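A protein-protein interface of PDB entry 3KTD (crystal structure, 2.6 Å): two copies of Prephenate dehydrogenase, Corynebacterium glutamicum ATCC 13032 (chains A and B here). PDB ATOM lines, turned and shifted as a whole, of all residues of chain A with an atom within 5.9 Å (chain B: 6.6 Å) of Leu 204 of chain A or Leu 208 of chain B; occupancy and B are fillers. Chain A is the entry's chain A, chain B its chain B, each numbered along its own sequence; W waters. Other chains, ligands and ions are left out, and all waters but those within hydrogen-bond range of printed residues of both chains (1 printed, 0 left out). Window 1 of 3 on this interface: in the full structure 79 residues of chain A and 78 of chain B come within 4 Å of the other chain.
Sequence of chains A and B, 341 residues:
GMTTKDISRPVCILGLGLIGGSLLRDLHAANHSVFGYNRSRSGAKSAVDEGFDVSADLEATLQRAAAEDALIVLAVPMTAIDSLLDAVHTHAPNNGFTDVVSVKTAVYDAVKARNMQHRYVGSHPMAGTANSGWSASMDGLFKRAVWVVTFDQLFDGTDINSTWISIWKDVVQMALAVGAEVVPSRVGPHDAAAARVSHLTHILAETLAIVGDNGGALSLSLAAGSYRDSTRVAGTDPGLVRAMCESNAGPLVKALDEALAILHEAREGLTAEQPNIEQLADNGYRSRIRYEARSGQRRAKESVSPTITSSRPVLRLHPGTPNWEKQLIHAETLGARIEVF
NH1 of Arg 196 of chain A is in hydrogen-bond range of O of Val 211 of chain B.
OG1 of Thr 201 of chain A sits at hydrogen-bond distance from O of Val 197 of chain A, 2.9 Å away. O of Ile 203 of chain A sits at hydrogen-bond distance from OG1 of Thr 207 of chain A (2.8 Å). O of Leu 208 of chain B lies within hydrogen-bond range of OH of Tyr 227 of chain B (3.4 Å). OH of Tyr 227 of chain B is in hydrogen-bond range of O of Ala 209 of chain B, 3.2 Å away. O of Ser 226 of chain B lies within hydrogen-bond range of OG of Ser 230 of chain B, at 2.7 Å. The backbone carbonyl oxygen (O) of Tyr 227 of chain B sits at hydrogen-bond distance from the side-chain hydroxyl (OG1) of Thr 231 of chain B (2.6 Å).
Among the printed residues, pairs that only touch across the chains: Thr 207 of chain A with Leu 263 of chain B (3.2 Å), Thr 201 of chain A with Ser 230 of chain B (3.4 Å), Leu 263 of chain A with Ile 203 of chain B (3.4 Å), Val 197 of chain A with Tyr 227 of chain B (3.4 Å), Thr 201 of chain A with Ser 226 of chain B (3.5 Å), Leu 263 of chain A with Thr 207 of chain B (3.6 Å), Thr 201 of chain A with Leu 208 of chain B (3.6 Å), Arg 196 of chain A with Leu 208 of chain B (3.6 Å), Ile 203 of chain A with Leu 263 of chain B (3.7 Å), Leu 200 of chain A with Val 211 of chain B (3.7 Å), Ile 203 of chain A with Leu 280 of chain B (3.7 Å), Thr 201 of chain A with Tyr 227 of chain B (3.7 Å), Leu 256 of chain A with Leu 263 of chain B (3.7 Å), Glu 206 of chain A with Leu 280 of chain B (3.8 Å), Ser 230 of chain A with Ser 230 of chain B (3.8 Å), Ala 259 of chain A with Thr 207 of chain B (3.8 Å), Leu 263 of chain A with Leu 263 of chain B (3.8 Å), Leu 204 of chain A with Leu 208 of chain B (3.9 Å), Ala 259 of chain A with Val 211 of chain B (3.9 Å) and Leu 204 of chain A with Leu 263 of chain B (3.96 Å).
Of the printed residues of chain B, Thr 201 of chain A touches Leu 208 (3.6 Å), Ser 226 (3.5 Å), Tyr 227 (3.7 Å) and Ser 230 (3.4 Å). Printed residues of chain B within 4 Å of Leu 204 of chain A: Leu 208 and Leu 263. Printed residues of chain B within 4 Å of Thr 207 of chain A: Leu 263. Ala 205 of chain B touches none of the printed residues of chain A. Of the printed residues of chain A, Leu 208 of chain B touches Arg 196 (3.6 Å), Thr 201 (3.6 Å) and Leu 204 (3.9 Å). Printed residues of chain A within 4 Å of Val 211 of chain B: Arg 196, Leu 200 and Ala 259. Thr 231 of chain B touches none of the printed residues of chain A. Printed residues of chain A within 4 Å of Leu 263 of chain B: Ile 203, Leu 204, Thr 207, Leu 256 and Leu 263. The nearest residue of chain B that does not touch Leu 204 of chain A is Leu 204 of chain B (4.1 Å). The nearest printed residue of chain B that does not touch Leu 263 of chain A is Leu 204 of chain B (4.1 Å).
Hydrophobic or aromatic side chains of chain B within 4 Å of the printed part of chain A: Ile 203, Leu 208, Val 211, Tyr 227, Leu 263 and Leu 280. Among the printed residues, 21 pairs touch across the chains.
Ile 203 of chain A touches Leu 263 of chain B, and with the chains exchanged Leu 263 of chain A touches Ile 203 of chain B. Thr 207 of chain A touches Leu 263 of chain B, and with the chains exchanged Leu 263 of chain A touches Thr 207 of chain B. Ser 230 of chain B touches its own counterpart, Ser 230 of chain A. Leu 263 of chain A touches its own counterpart, Leu 263 of chain B. Positions printed for both chains: 203, 204, 205, 206, 207, 208, 209, 230 and 263. Of the 21 pairs that touch across the chains among the printed residues, 6 have their exchanged pair printed and touching as well.
Water W1 bridges O of Val 197 of chain A (2.8 Å) and OG of Ser 226 of chain B (3.5 Å).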
ATOM      1  N   ARG A 196      15.138   4.787  24.917  1.00  0.00           N
ATOM      2  CA  ARG A 196      14.044   5.731  24.789  1.00  0.00           C
ATOM      3  C   ARG A 196      14.297   7.030  25.542  1.00  0.00           C
ATOM      4  O   ARG A 196      14.243   8.102  24.946  1.00  0.00           O
ATOM      5  CB  ARG A 196      12.751   5.104  25.302  1.00  0.00           C
ATOM      6  CG  ARG A 196      12.269   3.894  24.490  1.00  0.00           C
ATOM      7  CD  ARG A 196      11.099   3.192  25.187  1.00  0.00           C
ATOM      8  NE  ARG A 196      10.541   2.122  24.368  1.00  0.00           N
ATOM      9  CZ  ARG A 196       9.680   2.289  23.367  1.00  0.00           C
ATOM     10  NH1 ARG A 196       9.248   3.497  23.023  1.00  0.00           N
ATOM     11  NH2 ARG A 196       9.253   1.233  22.694  1.00  0.00           N
ATOM     12  N   VAL A 197      14.605   6.936  26.835  1.00  0.00           N
ATOM     13  CA  VAL A 197      14.635   8.127  27.687  1.00  0.00           C
ATOM     14  C   VAL A 197      15.968   8.862  27.794  1.00  0.00           C
ATOM     15  O   VAL A 197      16.034   9.948  28.384  1.00  0.00           O
ATOM     16  CB  VAL A 197      14.134   7.801  29.112  1.00  0.00           C
ATOM     17  CG1 VAL A 197      12.731   7.226  29.057  1.00  0.00           C
ATOM     18  CG2 VAL A 197      15.078   6.853  29.806  1.00  0.00           C
ATOM     19  N   HIS A 199      19.173   7.812  25.311  1.00  0.00           N
ATOM     20  CA  HIS A 199      19.931   7.725  24.072  1.00  0.00           C
ATOM     21  C   HIS A 199      19.221   8.464  22.932  1.00  0.00           C
ATOM     22  O   HIS A 199      19.834   9.298  22.285  1.00  0.00           O
ATOM     23  CB  HIS A 199      20.271   6.265  23.726  1.00  0.00           C
ATOM     24  CG  HIS A 199      20.987   5.538  24.832  1.00  0.00           C
ATOM     25  ND1 HIS A 199      20.932   4.170  24.993  1.00  0.00           N
ATOM     26  CD2 HIS A 199      21.733   6.004  25.863  1.00  0.00           C
ATOM     27  CE1 HIS A 199      21.641   3.824  26.051  1.00  0.00           C
ATOM     28  NE2 HIS A 199      22.137   4.920  26.597  1.00  0.00           N
ATOM     29  N   LEU A 200      17.935   8.196  22.714  1.00  0.00           N
ATOM     30  CA  LEU A 200      17.162   8.943  21.716  1.00  0.00           C
ATOM     31  C   LEU A 200      17.152  10.415  22.100  1.00  0.00           C
ATOM     32  O   LEU A 200      17.213  11.285  21.224  1.00  0.00           O
ATOM     33  CB  LEU A 200      15.724   8.425  21.620  1.00  0.00           C
ATOM     34  CG  LEU A 200      14.766   9.136  20.647  1.00  0.00           C
ATOM     35  CD1 LEU A 200      15.187   8.938  19.189  1.00  0.00           C
ATOM     36  CD2 LEU A 200      13.335   8.644  20.859  1.00  0.00           C
ATOM     37  N   THR A 201      17.088  10.693  23.409  1.00  0.00           N
ATOM     38  CA  THR A 201      17.111  12.075  23.898  1.00  0.00           C
ATOM     39  C   THR A 201      18.348  12.755  23.336  1.00  0.00           C
ATOM     40  O   THR A 201      18.271  13.853  22.766  1.00  0.00           O
ATOM     41  CB  THR A 201      17.112  12.153  25.435  1.00  0.00           C
ATOM     42  OG1 THR A 201      15.948  11.497  25.945  1.00  0.00           O
ATOM     43  CG2 THR A 201      17.130  13.610  25.928  1.00  0.00           C
ATOM     44  N   HIS A 202      19.484  12.077  23.463  1.00  0.00           N
ATOM     45  CA  HIS A 202      20.749  12.599  22.924  1.00  0.00           C
ATOM     46  C   HIS A 202      20.771  12.713  21.393  1.00  0.00           C
ATOM     47  O   HIS A 202      21.278  13.693  20.876  1.00  0.00           O
ATOM     48  CB  HIS A 202      21.935  11.779  23.430  1.00  0.00           C
ATOM     49  CG  HIS A 202      22.279  12.054  24.861  1.00  0.00           C
ATOM     50  ND1 HIS A 202      21.968  11.186  25.885  1.00  0.00           N
ATOM     51  CD2 HIS A 202      22.876  13.121  25.442  1.00  0.00           C
ATOM     52  CE1 HIS A 202      22.378  11.697  27.031  1.00  0.00           C
ATOM     53  NE2 HIS A 202      22.928  12.874  26.790  1.00  0.00           N
ATOM     54  N   ILE A 203      20.210  11.736  20.682  1.00  0.00           N
ATOM     55  CA  ILE A 203      20.181  11.776  19.225  1.00  0.00           C
ATOM     56  C   ILE A 203      19.358  12.974  18.731  1.00  0.00           C
ATOM     57  O   ILE A 203      19.792  13.700  17.845  1.00  0.00           O
ATOM     58  CB  ILE A 203      19.574  10.508  18.622  1.00  0.00           C
ATOM     59  CG1 ILE A 203      20.460   9.290  18.877  1.00  0.00           C
ATOM     60  CG2 ILE A 203      19.406  10.672  17.126  1.00  0.00           C
ATOM     61  CD1 ILE A 203      21.720   9.262  18.048  1.00  0.00           C
ATOM     62  N   LEU A 204      18.178  13.172  19.316  1.00  0.00           N
ATOM     63  CA  LEU A 204      17.301  14.275  18.946  1.00  0.00           C
ATOM     64  C   LEU A 204      17.943  15.622  19.269  1.00  0.00           C
ATOM     65  O   LEU A 204      17.788  16.583  18.512  1.00  0.00           O
ATOM     66  CB  LEU A 204      15.949  14.157  19.645  1.00  0.00           C
ATOM     67  CG  LEU A 204      15.103  12.918  19.325  1.00  0.00           C
ATOM     68  CD1 LEU A 204      13.844  12.898  20.153  1.00  0.00           C
ATOM     69  CD2 LEU A 204      14.755  12.844  17.852  1.00  0.00           C
ATOM     70  N   ALA A 205      18.670  15.683  20.384  1.00  0.00           N
ATOM     71  CA  ALA A 205      19.387  16.896  20.782  1.00  0.00           C
ATOM     72  C   ALA A 205      20.452  17.310  19.749  1.00  0.00           C
ATOM     73  O   ALA A 205      20.574  18.493  19.405  1.00  0.00           O
ATOM     74  CB  ALA A 205      20.016  16.697  22.130  1.00  0.00           C
ATOM     75  N   GLU A 206      21.213  16.340  19.247  1.00  0.00           N
ATOM     76  CA  GLU A 206      22.216  16.632  18.217  1.00  0.00           C
ATOM     77  C   GLU A 206      21.505  17.150  16.953  1.00  0.00           C
ATOM     78  O   GLU A 206      21.900  18.165  16.369  1.00  0.00           O
ATOM     79  CB  GLU A 206      23.036  15.386  17.835  1.00  0.00           C
ATOM     80  CG  GLU A 206      23.724  14.586  18.976  1.00  0.00           C
ATOM     81  CD  GLU A 206      24.878  15.301  19.674  1.00  0.00           C
ATOM     82  OE1 GLU A 206      25.007  16.545  19.581  1.00  0.00           O
ATOM     83  OE2 GLU A 206      25.653  14.593  20.349  1.00  0.00           O
ATOM     84  N   THR A 207      20.456  16.432  16.553  1.00  0.00           N
ATOM     85  CA  THR A 207      19.713  16.732  15.344  1.00  0.00           C
ATOM     86  C   THR A 207      19.186  18.157  15.351  1.00  0.00           C
ATOM     87  O   THR A 207      19.289  18.863  14.352  1.00  0.00           O
ATOM     88  CB  THR A 207      18.517  15.779  15.174  1.00  0.00           C
ATOM     89  OG1 THR A 207      18.958  14.422  15.305  1.00  0.00           O
ATOM     90  CG2 THR A 207      17.873  15.978  13.809  1.00  0.00           C
ATOM     91  N   LEU A 208      18.631  18.569  16.488  1.00  0.00           N
ATOM     92  CA  LEU A 208      18.044  19.893  16.631  1.00  0.00           C
ATOM     93  C   LEU A 208      19.112  20.968  16.529  1.00  0.00           C
ATOM     94  O   LEU A 208      18.887  22.010  15.916  1.00  0.00           O
ATOM     95  CB  LEU A 208      17.305  20.010  17.969  1.00  0.00           C
ATOM     96  CG  LEU A 208      16.684  21.384  18.263  1.00  0.00           C
ATOM     97  CD1 LEU A 208      15.628  21.734  17.222  1.00  0.00           C
ATOM     98  CD2 LEU A 208      16.107  21.453  19.679  1.00  0.00           C
ATOM     99  N   ALA A 209      20.276  20.723  17.125  1.00  0.00           N
ATOM    100  CA  ALA A 209      21.347  21.717  17.081  1.00  0.00           C
ATOM    101  C   ALA A 209      21.808  21.974  15.651  1.00  0.00           C
ATOM    102  O   ALA A 209      22.100  23.118  15.286  1.00  0.00           O
ATOM    103  CB  ALA A 209      22.513  21.307  17.953  1.00  0.00           C
ATOM    104  N   SER A 230      16.390  21.954  24.853  1.00  0.00           N
ATOM    105  CA  SER A 230      16.350  20.793  23.972  1.00  0.00           C
ATOM    106  C   SER A 230      17.678  20.484  23.306  1.00  0.00           C
ATOM    107  O   SER A 230      17.838  19.378  22.814  1.00  0.00           O
ATOM    108  CB  SER A 230      15.266  20.944  22.904  1.00  0.00           C
ATOM    109  OG  SER A 230      13.976  20.813  23.475  1.00  0.00           O
ATOM    110  N   LEU A 256      14.329   4.773  17.854  1.00  0.00           N
ATOM    111  CA  LEU A 256      14.409   5.784  16.804  1.00  0.00           C
ATOM    112  C   LEU A 256      13.350   5.568  15.710  1.00  0.00           C
ATOM    113  O   LEU A 256      12.833   6.537  15.154  1.00  0.00           O
ATOM    114  CB  LEU A 256      15.821   5.830  16.207  1.00  0.00           C
ATOM    115  CG  LEU A 256      16.137   6.869  15.118  1.00  0.00           C
ATOM    116  CD1 LEU A 256      15.730   8.266  15.526  1.00  0.00           C
ATOM    117  CD2 LEU A 256      17.617   6.842  14.786  1.00  0.00           C
ATOM    118  N   ALA A 259      10.228   7.037  16.779  1.00  0.00           N
ATOM    119  CA  ALA A 259      10.354   8.471  16.592  1.00  0.00           C
ATOM    120  C   ALA A 259      10.088   8.859  15.124  1.00  0.00           C
ATOM    121  O   ALA A 259       9.354   9.799  14.860  1.00  0.00           O
ATOM    122  CB  ALA A 259      11.718   8.931  17.025  1.00  0.00           C
ATOM    123  N   LEU A 263       7.055  11.129  13.660  1.00  0.00           N
ATOM    124  CA  LEU A 263       7.433  12.312  12.885  1.00  0.00           C
ATOM    125  C   LEU A 263       6.922  12.270  11.439  1.00  0.00           C
ATOM    126  O   LEU A 263       6.609  13.309  10.869  1.00  0.00           O
ATOM    127  CB  LEU A 263       8.953  12.520  12.903  1.00  0.00           C
ATOM    128  CG  LEU A 263       9.512  13.090  14.203  1.00  0.00           C
ATOM    129  CD1 LEU A 263      11.024  12.891  14.273  1.00  0.00           C
ATOM    130  CD2 LEU A 263       9.136  14.558  14.352  1.00  0.00           C
ATOM    131  N   ILE B 203       7.788  20.053  18.147  1.00  0.00           N
ATOM    132  CA  ILE B 203       7.537  18.782  17.469  1.00  0.00           C
ATOM    133  C   ILE B 203       8.420  17.678  18.033  1.00  0.00           C
ATOM    134  O   ILE B 203       7.936  16.609  18.373  1.00  0.00           O
ATOM    135  CB  ILE B 203       7.795  18.868  15.937  1.00  0.00           C
ATOM    136  CG1 ILE B 203       6.818  19.846  15.268  1.00  0.00           C
ATOM    137  CG2 ILE B 203       7.684  17.500  15.296  1.00  0.00           C
ATOM    138  CD1 ILE B 203       5.360  19.551  15.552  1.00  0.00           C
ATOM    139  N   LEU B 204       9.714  17.938  18.144  1.00  0.00           N
ATOM    140  CA  LEU B 204      10.636  16.920  18.636  1.00  0.00           C
ATOM    141  C   LEU B 204      10.386  16.567  20.097  1.00  0.00           C
ATOM    142  O   LEU B 204      10.576  15.424  20.490  1.00  0.00           O
ATOM    143  CB  LEU B 204      12.091  17.344  18.427  1.00  0.00           C
ATOM    144  CG  LEU B 204      12.522  17.554  16.972  1.00  0.00           C
ATOM    145  CD1 LEU B 204      13.944  18.069  16.978  1.00  0.00           C
ATOM    146  CD2 LEU B 204      12.385  16.278  16.105  1.00  0.00           C
ATOM    147  N   ALA B 205       9.947  17.531  20.897  1.00  0.00           N
ATOM    148  CA  ALA B 205       9.645  17.269  22.297  1.00  0.00           C
ATOM    149  C   ALA B 205       8.390  16.400  22.455  1.00  0.00           C
ATOM    150  O   ALA B 205       8.357  15.484  23.294  1.00  0.00           O
ATOM    151  CB  ALA B 205       9.482  18.563  23.046  1.00  0.00           C
ATOM    152  N   GLU B 206       7.354  16.692  21.673  1.00  0.00           N
ATOM    153  CA  GLU B 206       6.125  15.903  21.733  1.00  0.00           C
ATOM    154  C   GLU B 206       6.473  14.461  21.375  1.00  0.00           C
ATOM    155  O   GLU B 206       5.998  13.522  22.030  1.00  0.00           O
ATOM    156  CB  GLU B 206       5.029  16.430  20.774  1.00  0.00           C
ATOM    157  CG  GLU B 206       4.535  17.907  20.965  1.00  0.00           C
ATOM    158  CD  GLU B 206       3.697  18.141  22.215  1.00  0.00           C
ATOM    159  OE1 GLU B 206       3.877  17.423  23.219  1.00  0.00           O
ATOM    160  OE2 GLU B 206       2.865  19.069  22.205  1.00  0.00           O
ATOM    161  N   THR B 207       7.316  14.293  20.351  1.00  0.00           N
ATOM    162  CA  THR B 207       7.751  12.968  19.904  1.00  0.00           C
ATOM    163  C   THR B 207       8.512  12.210  20.989  1.00  0.00           C
ATOM    164  O   THR B 207       8.216  11.054  21.250  1.00  0.00           O
ATOM    165  CB  THR B 207       8.655  13.050  18.663  1.00  0.00           C
ATOM    166  OG1 THR B 207       7.961  13.718  17.613  1.00  0.00           O
ATOM    167  CG2 THR B 207       9.045  11.666  18.183  1.00  0.00           C
ATOM    168  N   LEU B 208       9.492  12.848  21.612  1.00  0.00           N
ATOM    169  CA  LEU B 208      10.289  12.186  22.647  1.00  0.00           C
ATOM    170  C   LEU B 208       9.394  11.746  23.806  1.00  0.00           C
ATOM    171  O   LEU B 208       9.458  10.602  24.255  1.00  0.00           O
ATOM    172  CB  LEU B 208      11.408  13.112  23.147  1.00  0.00           C
ATOM    173  CG  LEU B 208      12.363  12.611  24.242  1.00  0.00           C
ATOM    174  CD1 LEU B 208      13.053  11.307  23.843  1.00  0.00           C
ATOM    175  CD2 LEU B 208      13.398  13.682  24.548  1.00  0.00           C
ATOM    176  N   ALA B 209       8.539  12.653  24.265  1.00  0.00           N
ATOM    177  CA  ALA B 209       7.590  12.353  25.335  1.00  0.00           C
ATOM    178  C   ALA B 209       6.789  11.069  25.080  1.00  0.00           C
ATOM    179  O   ALA B 209       6.612  10.262  25.995  1.00  0.00           O
ATOM    180  CB  ALA B 209       6.650  13.522  25.533  1.00  0.00           C
ATOM    181  N   ILE B 210       6.320  10.889  23.842  1.00  0.00           N
ATOM    182  CA  ILE B 210       5.520   9.731  23.466  1.00  0.00           C
ATOM    183  C   ILE B 210       6.370   8.477  23.420  1.00  0.00           C
ATOM    184  O   ILE B 210       5.977   7.428  23.953  1.00  0.00           O
ATOM    185  CB  ILE B 210       4.866   9.913  22.085  1.00  0.00           C
ATOM    186  CG1 ILE B 210       3.832  11.037  22.115  1.00  0.00           C
ATOM    187  CG2 ILE B 210       4.169   8.634  21.627  1.00  0.00           C
ATOM    188  CD1 ILE B 210       3.328  11.426  20.722  1.00  0.00           C
ATOM    189  N   VAL B 211       7.532   8.563  22.774  1.00  0.00           N
ATOM    190  CA  VAL B 211       8.402   7.399  22.701  1.00  0.00           C
ATOM    191  C   VAL B 211       8.721   6.905  24.109  1.00  0.00           C
ATOM    192  O   VAL B 211       8.626   5.714  24.384  1.00  0.00           O
ATOM    193  CB  VAL B 211       9.698   7.672  21.957  1.00  0.00           C
ATOM    194  CG1 VAL B 211      10.656   6.472  22.124  1.00  0.00           C
ATOM    195  CG2 VAL B 211       9.414   7.946  20.489  1.00  0.00           C
ATOM    196  N   GLY B 212       9.067   7.827  25.002  1.00  0.00           N
ATOM    197  CA  GLY B 212       9.361   7.477  26.392  1.00  0.00           C
ATOM    198  C   GLY B 212       8.160   6.878  27.103  1.00  0.00           C
ATOM    199  O   GLY B 212       8.300   5.947  27.899  1.00  0.00           O
ATOM    200  N   ASP B 213       6.973   7.407  26.813  1.00  0.00           N
ATOM    201  CA  ASP B 213       5.746   6.904  27.418  1.00  0.00           C
ATOM    202  C   ASP B 213       5.388   5.517  26.872  1.00  0.00           C
ATOM    203  O   ASP B 213       4.811   4.701  27.584  1.00  0.00           O
ATOM    204  CB  ASP B 213       4.600   7.885  27.171  1.00  0.00           C
ATOM    205  CG  ASP B 213       3.331   7.502  27.909  1.00  0.00           C
ATOM    206  OD1 ASP B 213       3.348   7.449  29.148  1.00  0.00           O
ATOM    207  OD2 ASP B 213       2.305   7.262  27.250  1.00  0.00           O
ATOM    208  N   SER B 226      18.242  14.832  31.145  1.00  0.00           N
ATOM    209  CA  SER B 226      18.178  15.156  29.723  1.00  0.00           C
ATOM    210  C   SER B 226      16.748  15.069  29.190  1.00  0.00           C
ATOM    211  O   SER B 226      16.311  15.921  28.398  1.00  0.00           O
ATOM    212  CB  SER B 226      19.096  14.242  28.915  1.00  0.00           C
ATOM    213  OG  SER B 226      18.713  12.888  29.045  1.00  0.00           O
ATOM    214  N   TYR B 227      16.028  14.042  29.634  1.00  0.00           N
ATOM    215  CA  TYR B 227      14.657  13.811  29.199  1.00  0.00           C
ATOM    216  C   TYR B 227      13.766  14.919  29.711  1.00  0.00           C
ATOM    217  O   TYR B 227      12.967  15.499  28.961  1.00  0.00           O
ATOM    218  CB  TYR B 227      14.174  12.483  29.741  1.00  0.00           C
ATOM    219  CG  TYR B 227      12.865  11.996  29.184  1.00  0.00           C
ATOM    220  CD1 TYR B 227      12.794  11.461  27.907  1.00  0.00           C
ATOM    221  CD2 TYR B 227      11.712  12.017  29.949  1.00  0.00           C
ATOM    222  CE1 TYR B 227      11.602  10.983  27.401  1.00  0.00           C
ATOM    223  CE2 TYR B 227      10.524  11.531  29.457  1.00  0.00           C
ATOM    224  CZ  TYR B 227      10.470  11.022  28.179  1.00  0.00           C
ATOM    225  OH  TYR B 227       9.282  10.543  27.674  1.00  0.00           O
ATOM    226  N   SER B 230      14.429  18.065  27.688  1.00  0.00           N
ATOM    227  CA  SER B 230      14.054  17.966  26.260  1.00  0.00           C
ATOM    228  C   SER B 230      12.567  17.722  26.009  1.00  0.00           C
ATOM    229  O   SER B 230      12.121  17.812  24.869  1.00  0.00           O
ATOM    230  CB  SER B 230      14.854  16.851  25.566  1.00  0.00           C
ATOM    231  OG  SER B 230      16.231  16.893  25.912  1.00  0.00           O
ATOM    232  N   THR B 231      11.815  17.388  27.053  1.00  0.00           N
ATOM    233  CA  THR B 231      10.375  17.152  26.937  1.00  0.00           C
ATOM    234  C   THR B 231       9.590  18.249  27.670  1.00  0.00           C
ATOM    235  O   THR B 231       8.377  18.134  27.842  1.00  0.00           O
ATOM    236  CB  THR B 231       9.974  15.768  27.530  1.00  0.00           C
ATOM    237  OG1 THR B 231      10.369  15.683  28.913  1.00  0.00           O
ATOM    238  CG2 THR B 231      10.621  14.645  26.756  1.00  0.00           C
ATOM    239  N   LEU B 263      18.228  12.212  10.995  1.00  0.00           N
ATOM    240  CA  LEU B 263      17.806  11.077  11.797  1.00  0.00           C
ATOM    241  C   LEU B 263      17.922   9.743  11.043  1.00  0.00           C
ATOM    242  O   LEU B 263      18.322   8.732  11.638  1.00  0.00           O
ATOM    243  CB  LEU B 263      16.390  11.311  12.351  1.00  0.00           C
ATOM    244  CG  LEU B 263      16.276  12.399  13.436  1.00  0.00           C
ATOM    245  CD1 LEU B 263      14.825  12.731  13.754  1.00  0.00           C
ATOM    246  CD2 LEU B 263      17.008  11.985  14.707  1.00  0.00           C
ATOM    247  N   LEU B 280      26.979  12.549  13.269  1.00  0.00           N
ATOM    248  CA  LEU B 280      25.943  13.196  14.066  1.00  0.00           C
ATOM    249  C   LEU B 280      26.498  13.832  15.331  1.00  0.00           C
ATOM    250  O   LEU B 280      26.279  15.019  15.584  1.00  0.00           O
ATOM    251  CB  LEU B 280      24.852  12.194  14.445  1.00  0.00           C
ATOM    252  CG  LEU B 280      23.633  12.815  15.131  1.00  0.00           C
ATOM    253  CD1 LEU B 280      23.033  13.879  14.233  1.00  0.00           C
ATOM    254  CD2 LEU B 280      22.600  11.757  15.492  1.00  0.00           C
HETATM  255  O   HOH W   1      16.977  10.497  30.913  1.00  0.00           O
